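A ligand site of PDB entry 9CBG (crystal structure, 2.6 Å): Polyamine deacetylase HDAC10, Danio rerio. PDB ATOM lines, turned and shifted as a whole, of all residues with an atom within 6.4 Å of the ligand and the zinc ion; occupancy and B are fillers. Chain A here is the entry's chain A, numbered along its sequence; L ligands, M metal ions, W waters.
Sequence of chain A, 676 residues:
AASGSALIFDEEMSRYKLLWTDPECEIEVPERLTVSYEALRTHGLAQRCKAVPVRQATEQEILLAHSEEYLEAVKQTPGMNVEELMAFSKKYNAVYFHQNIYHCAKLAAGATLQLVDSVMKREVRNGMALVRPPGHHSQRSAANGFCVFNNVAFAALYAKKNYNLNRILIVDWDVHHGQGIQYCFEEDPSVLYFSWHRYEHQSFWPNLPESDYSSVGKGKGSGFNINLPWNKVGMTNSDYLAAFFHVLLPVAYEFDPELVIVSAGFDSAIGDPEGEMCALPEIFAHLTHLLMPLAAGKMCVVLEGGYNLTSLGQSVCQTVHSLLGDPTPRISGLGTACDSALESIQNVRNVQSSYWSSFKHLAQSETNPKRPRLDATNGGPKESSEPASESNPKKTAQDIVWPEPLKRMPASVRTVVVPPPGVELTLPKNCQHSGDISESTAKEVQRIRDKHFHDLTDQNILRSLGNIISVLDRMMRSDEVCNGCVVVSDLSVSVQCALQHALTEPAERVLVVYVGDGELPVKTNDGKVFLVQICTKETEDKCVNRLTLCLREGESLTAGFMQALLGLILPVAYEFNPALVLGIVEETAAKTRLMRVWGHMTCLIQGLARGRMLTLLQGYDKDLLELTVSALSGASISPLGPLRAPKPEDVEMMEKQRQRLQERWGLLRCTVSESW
N1 of the ligand is in salt-bridge range of OE1 of Glu 274 (3.0 Å). A ring nitrogen (NE2) of His 137 sits close to a sulfur (S1) of the ligand, 3.4 Å away. The side-chain hydroxyl of Tyr 307 is in hydrogen-bond range of an oxygen (O1) of the ligand. S1 of the ligand lies close to NE2 of His 136, 3.1 Å away.
The backbone NH of His 136 is in hydrogen-bond range of the side-chain carboxylate of Glu 304, at 3.0 Å. N of His 137 is in hydrogen-bond range of SG of Cys 147, 3.5 Å away. OD1 of Asn 93 sits at hydrogen-bond distance from NE1 of Trp 205, 2.6 Å away. N of Gly 145 is in hydrogen-bond range of O of Asn 93 (3.4 Å). N of Val 175 is in hydrogen-bond range of OD1 of Asp 267. The backbone NH of Gly 145 is in hydrogen-bond range of the backbone carbonyl oxygen of Ala 94, 3.3 Å away. The backbone NH (N) of His 136 is in hydrogen-bond range of the side-chain sulfur (SG) of Cys 147, 3.6 Å away. A ring nitrogen (NE2) of His 137 sits at hydrogen-bond distance from a ring nitrogen (NE2) of His 136.
Glu 24 touches the ligand. Ala 94 touches the ligand (CB to C9, 3.6 Å). Gly 145 touches the ligand. Phe 146 touches the ligand (CE2 to C3, 3.3 Å). Trp 205 touches the ligand. Of the 25 residues printed, 12 come within 4 Å of the ligand.
The zinc ion is bound by OD1 of Asp 174 (2.0 Å), OD2 of Asp 267 (2.0 Å), ND1 of His 176 (2.1 Å) and S1 of the ligand (2.2 Å). Slightly farther from the zinc ion lies the side-chain carboxylate (OD2) of Asp 174 (2.6 Å).
Water W1 lies within hydrogen-bond range of a nitrogen (N1) of the ligand (2.8 Å), the backbone carbonyl oxygen of Glu 24 (3.2 Å) and the backbone carbonyl oxygen of Pro 23 (3.4 Å).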
ATOM      1  N   PRO A  23     -33.508  16.522   4.197  1.00  0.00           N
ATOM      2  CA  PRO A  23     -33.507  16.811   2.750  1.00  0.00           C
ATOM      3  C   PRO A  23     -32.121  17.082   2.188  1.00  0.00           C
ATOM      4  O   PRO A  23     -31.946  17.018   0.964  1.00  0.00           O
ATOM      5  CB  PRO A  23     -34.409  18.041   2.635  1.00  0.00           C
ATOM      6  CG  PRO A  23     -35.250  18.019   3.880  1.00  0.00           C
ATOM      7  CD  PRO A  23     -34.347  17.470   4.945  1.00  0.00           C
ATOM      8  N   GLU A  24     -31.134  17.353   3.040  1.00  0.00           N
ATOM      9  CA  GLU A  24     -29.783  17.605   2.554  1.00  0.00           C
ATOM     10  C   GLU A  24     -29.076  16.311   2.160  1.00  0.00           C
ATOM     11  O   GLU A  24     -28.292  16.306   1.196  1.00  0.00           O
ATOM     12  CB  GLU A  24     -28.980  18.341   3.611  1.00  0.00           C
ATOM     13  CG  GLU A  24     -27.672  18.917   3.116  1.00  0.00           C
ATOM     14  CD  GLU A  24     -26.991  19.735   4.184  1.00  0.00           C
ATOM     15  OE1 GLU A  24     -27.150  19.385   5.375  1.00  0.00           O
ATOM     16  OE2 GLU A  24     -26.310  20.723   3.851  1.00  0.00           O
ATOM     17  N   CYS A  25     -29.320  15.222   2.881  1.00  0.00           N
ATOM     18  CA  CYS A  25     -28.657  13.942   2.648  1.00  0.00           C
ATOM     19  C   CYS A  25     -29.536  12.929   1.927  1.00  0.00           C
ATOM     20  O   CYS A  25     -29.106  11.782   1.732  1.00  0.00           O
ATOM     21  CB  CYS A  25     -28.165  13.355   3.972  1.00  0.00           C
ATOM     22  SG  CYS A  25     -26.868  14.280   4.829  1.00  0.00           S
ATOM     23  N   ILE A  27     -30.220  12.422  -1.052  1.00  0.00           N
ATOM     24  CA  ILE A  27     -29.789  11.952  -2.362  1.00  0.00           C
ATOM     25  C   ILE A  27     -28.805  10.785  -2.245  1.00  0.00           C
ATOM     26  O   ILE A  27     -28.704   9.974  -3.170  1.00  0.00           O
ATOM     27  CB  ILE A  27     -29.163  13.107  -3.165  1.00  0.00           C
ATOM     28  CG1 ILE A  27     -28.024  13.756  -2.371  1.00  0.00           C
ATOM     29  CG2 ILE A  27     -30.226  14.119  -3.570  1.00  0.00           C
ATOM     30  CD1 ILE A  27     -27.173  14.714  -3.173  1.00  0.00           C
ATOM     31  N   ASN A  93     -21.310  18.594   9.369  1.00  0.00           N
ATOM     32  CA  ASN A  93     -22.105  19.272   8.349  1.00  0.00           C
ATOM     33  C   ASN A  93     -22.345  18.329   7.176  1.00  0.00           C
ATOM     34  O   ASN A  93     -21.392  17.844   6.561  1.00  0.00           O
ATOM     35  CB  ASN A  93     -21.426  20.562   7.882  1.00  0.00           C
ATOM     36  CG  ASN A  93     -22.104  21.174   6.671  1.00  0.00           C
ATOM     37  OD1 ASN A  93     -21.517  21.269   5.599  1.00  0.00           O
ATOM     38  ND2 ASN A  93     -23.364  21.561   6.838  1.00  0.00           N
ATOM     39  N   ALA A  94     -23.623  18.050   6.904  1.00  0.00           N
ATOM     40  CA  ALA A  94     -24.060  17.308   5.714  1.00  0.00           C
ATOM     41  C   ALA A  94     -23.579  15.853   5.717  1.00  0.00           C
ATOM     42  O   ALA A  94     -23.007  15.365   4.741  1.00  0.00           O
ATOM     43  CB  ALA A  94     -23.635  18.029   4.438  1.00  0.00           C
ATOM     44  N   PRO A 134     -18.478   7.864   0.152  1.00  0.00           N
ATOM     45  CA  PRO A 134     -17.425   8.631  -0.522  1.00  0.00           C
ATOM     46  C   PRO A 134     -16.376   9.140   0.458  1.00  0.00           C
ATOM     47  O   PRO A 134     -16.467   8.899   1.669  1.00  0.00           O
ATOM     48  CB  PRO A 134     -18.185   9.790  -1.172  1.00  0.00           C
ATOM     49  CG  PRO A 134     -19.632   9.455  -1.077  1.00  0.00           C
ATOM     50  CD  PRO A 134     -19.777   8.554   0.114  1.00  0.00           C
ATOM     51  N   HIS A 136     -13.891  12.281  -0.520  1.00  0.00           N
ATOM     52  CA  HIS A 136     -13.059  13.460  -0.809  1.00  0.00           C
ATOM     53  C   HIS A 136     -13.375  14.656   0.077  1.00  0.00           C
ATOM     54  O   HIS A 136     -12.597  15.623   0.066  1.00  0.00           O
ATOM     55  CB  HIS A 136     -13.155  13.851  -2.293  1.00  0.00           C
ATOM     56  CG  HIS A 136     -14.505  14.352  -2.715  1.00  0.00           C
ATOM     57  ND1 HIS A 136     -14.668  15.280  -3.715  1.00  0.00           N
ATOM     58  CD2 HIS A 136     -15.756  14.014  -2.306  1.00  0.00           C
ATOM     59  CE1 HIS A 136     -15.955  15.514  -3.899  1.00  0.00           C
ATOM     60  NE2 HIS A 136     -16.633  14.756  -3.054  1.00  0.00           N
ATOM     61  N   HIS A 137     -14.463  14.631   0.842  1.00  0.00           N
ATOM     62  CA  HIS A 137     -14.799  15.729   1.738  1.00  0.00           C
ATOM     63  C   HIS A 137     -14.310  15.511   3.168  1.00  0.00           C
ATOM     64  O   HIS A 137     -14.092  16.500   3.886  1.00  0.00           O
ATOM     65  CB  HIS A 137     -16.315  15.960   1.770  1.00  0.00           C
ATOM     66  CG  HIS A 137     -16.860  16.497   0.487  1.00  0.00           C
ATOM     67  ND1 HIS A 137     -16.473  17.727  -0.026  1.00  0.00           N
ATOM     68  CD2 HIS A 137     -17.757  15.992  -0.393  1.00  0.00           C
ATOM     69  CE1 HIS A 137     -17.099  17.939  -1.164  1.00  0.00           C
ATOM     70  NE2 HIS A 137     -17.885  16.905  -1.412  1.00  0.00           N
ATOM     71  N   ASN A 144     -17.549  14.779   6.690  1.00  0.00           N
ATOM     72  CA  ASN A 144     -18.156  15.925   5.967  1.00  0.00           C
ATOM     73  C   ASN A 144     -18.642  15.486   4.601  1.00  0.00           C
ATOM     74  O   ASN A 144     -17.971  14.651   3.991  1.00  0.00           O
ATOM     75  CB  ASN A 144     -17.134  17.058   5.825  1.00  0.00           C
ATOM     76  CG  ASN A 144     -17.721  18.327   5.275  1.00  0.00           C
ATOM     77  OD1 ASN A 144     -17.323  18.767   4.193  1.00  0.00           O
ATOM     78  ND2 ASN A 144     -18.660  18.926   5.996  1.00  0.00           N
ATOM     79  N   GLY A 145     -19.785  15.995   4.157  1.00  0.00           N
ATOM     80  CA  GLY A 145     -20.248  15.720   2.779  1.00  0.00           C
ATOM     81  C   GLY A 145     -20.405  14.257   2.493  1.00  0.00           C
ATOM     82  O   GLY A 145     -19.735  13.774   1.566  1.00  0.00           O
ATOM     83  N   PHE A 146     -21.253  13.581   3.261  1.00  0.00           N
ATOM     84  CA  PHE A 146     -21.549  12.144   3.016  1.00  0.00           C
ATOM     85  C   PHE A 146     -20.272  11.322   3.123  1.00  0.00           C
ATOM     86  O   PHE A 146     -20.303  10.143   2.758  1.00  0.00           O
ATOM     87  CB  PHE A 146     -22.208  11.954   1.654  1.00  0.00           C
ATOM     88  CG  PHE A 146     -23.317  12.901   1.217  1.00  0.00           C
ATOM     89  CD1 PHE A 146     -24.185  13.473   2.139  1.00  0.00           C
ATOM     90  CD2 PHE A 146     -23.501  13.196  -0.128  1.00  0.00           C
ATOM     91  CE1 PHE A 146     -25.194  14.321   1.726  1.00  0.00           C
ATOM     92  CE2 PHE A 146     -24.509  14.053  -0.530  1.00  0.00           C
ATOM     93  CZ  PHE A 146     -25.353  14.602   0.390  1.00  0.00           C
ATOM     94  N   CYS A 147     -19.180  11.909   3.612  1.00  0.00           N
ATOM     95  CA  CYS A 147     -17.918  11.190   3.670  1.00  0.00           C
ATOM     96  C   CYS A 147     -17.517  10.913   5.113  1.00  0.00           C
ATOM     97  O   CYS A 147     -17.681  11.775   5.994  1.00  0.00           O
ATOM     98  CB  CYS A 147     -16.789  11.971   2.966  1.00  0.00           C
ATOM     99  SG  CYS A 147     -17.039  12.265   1.201  1.00  0.00           S
ATOM    100  N   ASP A 174     -15.518  15.553  -9.551  1.00  0.00           N
ATOM    101  CA  ASP A 174     -16.785  15.781  -8.858  1.00  0.00           C
ATOM    102  C   ASP A 174     -17.092  17.283  -8.819  1.00  0.00           C
ATOM    103  O   ASP A 174     -16.166  18.102  -8.739  1.00  0.00           O
ATOM    104  CB  ASP A 174     -16.677  15.222  -7.438  1.00  0.00           C
ATOM    105  CG  ASP A 174     -18.016  15.113  -6.729  1.00  0.00           C
ATOM    106  OD1 ASP A 174     -18.671  16.146  -6.503  1.00  0.00           O
ATOM    107  OD2 ASP A 174     -18.403  13.987  -6.398  1.00  0.00           O
ATOM    108  N   VAL A 175     -18.384  17.653  -8.886  1.00  0.00           N
ATOM    109  CA  VAL A 175     -18.729  19.080  -8.871  1.00  0.00           C
ATOM    110  C   VAL A 175     -18.429  19.728  -7.539  1.00  0.00           C
ATOM    111  O   VAL A 175     -18.465  20.959  -7.434  1.00  0.00           O
ATOM    112  CB  VAL A 175     -20.207  19.387  -9.179  1.00  0.00           C
ATOM    113  CG1 VAL A 175     -20.516  19.336 -10.663  1.00  0.00           C
ATOM    114  CG2 VAL A 175     -21.118  18.500  -8.355  1.00  0.00           C
ATOM    115  N   HIS A 176     -18.111  18.896  -6.555  1.00  0.00           N
ATOM    116  CA  HIS A 176     -17.791  19.418  -5.212  1.00  0.00           C
ATOM    117  C   HIS A 176     -16.272  19.442  -5.050  1.00  0.00           C
ATOM    118  O   HIS A 176     -15.570  18.737  -5.802  1.00  0.00           O
ATOM    119  CB  HIS A 176     -18.552  18.614  -4.150  1.00  0.00           C
ATOM    120  CG  HIS A 176     -20.019  18.605  -4.340  1.00  0.00           C
ATOM    121  ND1 HIS A 176     -20.733  17.622  -5.003  1.00  0.00           N
ATOM    122  CD2 HIS A 176     -20.920  19.492  -3.923  1.00  0.00           C
ATOM    123  CE1 HIS A 176     -22.016  17.958  -4.995  1.00  0.00           C
ATOM    124  NE2 HIS A 176     -22.148  19.074  -4.325  1.00  0.00           N
ATOM    125  N   PHE A 204     -21.991  28.267  -3.052  1.00  0.00           N
ATOM    126  CA  PHE A 204     -22.341  26.857  -3.164  1.00  0.00           C
ATOM    127  C   PHE A 204     -21.518  26.005  -2.206  1.00  0.00           C
ATOM    128  O   PHE A 204     -20.348  26.303  -1.909  1.00  0.00           O
ATOM    129  CB  PHE A 204     -22.138  26.358  -4.600  1.00  0.00           C
ATOM    130  CG  PHE A 204     -22.686  24.977  -4.843  1.00  0.00           C
ATOM    131  CD1 PHE A 204     -24.043  24.793  -5.037  1.00  0.00           C
ATOM    132  CD2 PHE A 204     -21.851  23.872  -4.872  1.00  0.00           C
ATOM    133  CE1 PHE A 204     -24.563  23.527  -5.261  1.00  0.00           C
ATOM    134  CE2 PHE A 204     -22.355  22.601  -5.094  1.00  0.00           C
ATOM    135  CZ  PHE A 204     -23.723  22.436  -5.292  1.00  0.00           C
ATOM    136  N   TRP A 205     -22.134  24.914  -1.738  1.00  0.00           N
ATOM    137  CA  TRP A 205     -21.531  24.074  -0.716  1.00  0.00           C
ATOM    138  C   TRP A 205     -20.194  23.524  -1.210  1.00  0.00           C
ATOM    139  O   TRP A 205     -20.080  23.107  -2.368  1.00  0.00           O
ATOM    140  CB  TRP A 205     -22.473  22.933  -0.343  1.00  0.00           C
ATOM    141  CG  TRP A 205     -22.042  22.230   0.899  1.00  0.00           C
ATOM    142  CD1 TRP A 205     -22.453  22.498   2.174  1.00  0.00           C
ATOM    143  CD2 TRP A 205     -21.097  21.164   0.992  1.00  0.00           C
ATOM    144  NE1 TRP A 205     -21.820  21.667   3.054  1.00  0.00           N
ATOM    145  CE2 TRP A 205     -20.975  20.840   2.360  1.00  0.00           C
ATOM    146  CE3 TRP A 205     -20.335  20.466   0.059  1.00  0.00           C
ATOM    147  CZ2 TRP A 205     -20.125  19.835   2.813  1.00  0.00           C
ATOM    148  CZ3 TRP A 205     -19.494  19.469   0.506  1.00  0.00           C
ATOM    149  CH2 TRP A 205     -19.391  19.160   1.873  1.00  0.00           C
ATOM    150  N   GLY A 265     -16.455  11.500  -9.242  1.00  0.00           N
ATOM    151  CA  GLY A 265     -17.780  11.970  -8.915  1.00  0.00           C
ATOM    152  C   GLY A 265     -18.523  12.337 -10.170  1.00  0.00           C
ATOM    153  O   GLY A 265     -18.119  13.259 -10.888  1.00  0.00           O
ATOM    154  N   ASP A 267     -21.598  13.512 -10.398  1.00  0.00           N
ATOM    155  CA  ASP A 267     -22.583  14.593 -10.276  1.00  0.00           C
ATOM    156  C   ASP A 267     -22.239  15.787 -11.153  1.00  0.00           C
ATOM    157  O   ASP A 267     -23.004  16.757 -11.185  1.00  0.00           O
ATOM    158  CB  ASP A 267     -22.728  15.032  -8.815  1.00  0.00           C
ATOM    159  CG  ASP A 267     -21.400  15.249  -8.116  1.00  0.00           C
ATOM    160  OD1 ASP A 267     -20.352  15.228  -8.791  1.00  0.00           O
ATOM    161  OD2 ASP A 267     -21.411  15.449  -6.878  1.00  0.00           O
ATOM    162  N   GLU A 274     -27.758  17.753  -8.194  1.00  0.00           N
ATOM    163  CA  GLU A 274     -26.885  18.523  -7.322  1.00  0.00           C
ATOM    164  C   GLU A 274     -25.948  19.428  -8.127  1.00  0.00           C
ATOM    165  O   GLU A 274     -25.814  20.614  -7.817  1.00  0.00           O
ATOM    166  CB  GLU A 274     -26.096  17.574  -6.425  1.00  0.00           C
ATOM    167  CG  GLU A 274     -25.308  18.263  -5.325  1.00  0.00           C
ATOM    168  CD  GLU A 274     -26.204  18.897  -4.285  1.00  0.00           C
ATOM    169  OE1 GLU A 274     -27.293  18.352  -4.000  1.00  0.00           O
ATOM    170  OE2 GLU A 274     -25.812  19.960  -3.753  1.00  0.00           O
ATOM    171  N   GLU A 304     -16.945   8.722  -6.185  1.00  0.00           N
ATOM    172  CA  GLU A 304     -17.204   9.757  -5.161  1.00  0.00           C
ATOM    173  C   GLU A 304     -18.694  10.118  -5.234  1.00  0.00           C
ATOM    174  O   GLU A 304     -19.481   9.497  -4.510  1.00  0.00           O
ATOM    175  CB  GLU A 304     -16.307  10.965  -5.371  1.00  0.00           C
ATOM    176  CG  GLU A 304     -14.835  10.684  -5.095  1.00  0.00           C
ATOM    177  CD  GLU A 304     -14.434  10.722  -3.639  1.00  0.00           C
ATOM    178  OE1 GLU A 304     -15.303  10.935  -2.775  1.00  0.00           O
ATOM    179  OE2 GLU A 304     -13.236  10.543  -3.360  1.00  0.00           O
ATOM    180  N   GLY A 305     -19.067  11.059  -6.107  1.00  0.00           N
ATOM    181  CA  GLY A 305     -20.461  11.519  -6.164  1.00  0.00           C
ATOM    182  C   GLY A 305     -21.215  11.055  -7.384  1.00  0.00           C
ATOM    183  O   GLY A 305     -20.666  10.250  -8.144  1.00  0.00           O
ATOM    184  N   GLY A 306     -22.428  11.559  -7.573  1.00  0.00           N
ATOM    185  CA  GLY A 306     -23.301  11.116  -8.648  1.00  0.00           C
ATOM    186  C   GLY A 306     -24.633  10.577  -8.162  1.00  0.00           C
ATOM    187  O   GLY A 306     -24.695   9.463  -7.610  1.00  0.00           O
ATOM    188  N   TYR A 307     -25.718  11.334  -8.385  1.00  0.00           N
ATOM    189  CA  TYR A 307     -26.991  11.043  -7.725  1.00  0.00           C
ATOM    190  C   TYR A 307     -28.188  10.958  -8.655  1.00  0.00           C
ATOM    191  O   TYR A 307     -29.312  10.763  -8.179  1.00  0.00           O
ATOM    192  CB  TYR A 307     -27.252  12.084  -6.631  1.00  0.00           C
ATOM    193  CG  TYR A 307     -26.046  12.257  -5.740  1.00  0.00           C
ATOM    194  CD1 TYR A 307     -25.842  11.423  -4.647  1.00  0.00           C
ATOM    195  CD2 TYR A 307     -25.097  13.243  -5.991  1.00  0.00           C
ATOM    196  CE1 TYR A 307     -24.737  11.572  -3.826  1.00  0.00           C
ATOM    197  CE2 TYR A 307     -23.992  13.405  -5.181  1.00  0.00           C
ATOM    198  CZ  TYR A 307     -23.819  12.563  -4.106  1.00  0.00           C
ATOM    199  OH  TYR A 307     -22.709  12.739  -3.299  1.00  0.00           O
HETATM  200  C1  LIG L   1     -22.049  15.749  -2.197  1.00  0.00           C
HETATM  201  C2  LIG L   1     -20.832  14.885  -1.852  1.00  0.00           C
HETATM  202  C3  LIG L   1     -22.587  16.725  -1.145  1.00  0.00           C
HETATM  203  C4  LIG L   1     -23.669  17.548  -1.416  1.00  0.00           C
HETATM  204  C5  LIG L   1     -24.128  18.430  -0.442  1.00  0.00           C
HETATM  205  C6  LIG L   1     -25.313  19.347  -0.724  1.00  0.00           C
HETATM  206  C7  LIG L   1     -26.673  18.698  -0.485  1.00  0.00           C
HETATM  207  C8  LIG L   1     -23.506  18.489   0.802  1.00  0.00           C
HETATM  208  C9  LIG L   1     -22.429  17.666   1.064  1.00  0.00           C
HETATM  209  C10 LIG L   1     -21.965  16.784   0.099  1.00  0.00           C
HETATM  210  N1  LIG L   1     -27.686  19.419  -1.227  1.00  0.00           N
HETATM  211  O1  LIG L   1     -22.560  15.662  -3.262  1.00  0.00           O
HETATM  212  S1  LIG L   1     -19.700  14.748  -3.258  1.00  0.00           S
HETATM  213 ZN    ZN M   1     -20.158  15.575  -5.282  1.00  0.00          ZN
HETATM  214  O   HOH W   1     -29.618  17.388  -1.481  1.00  0.00           O
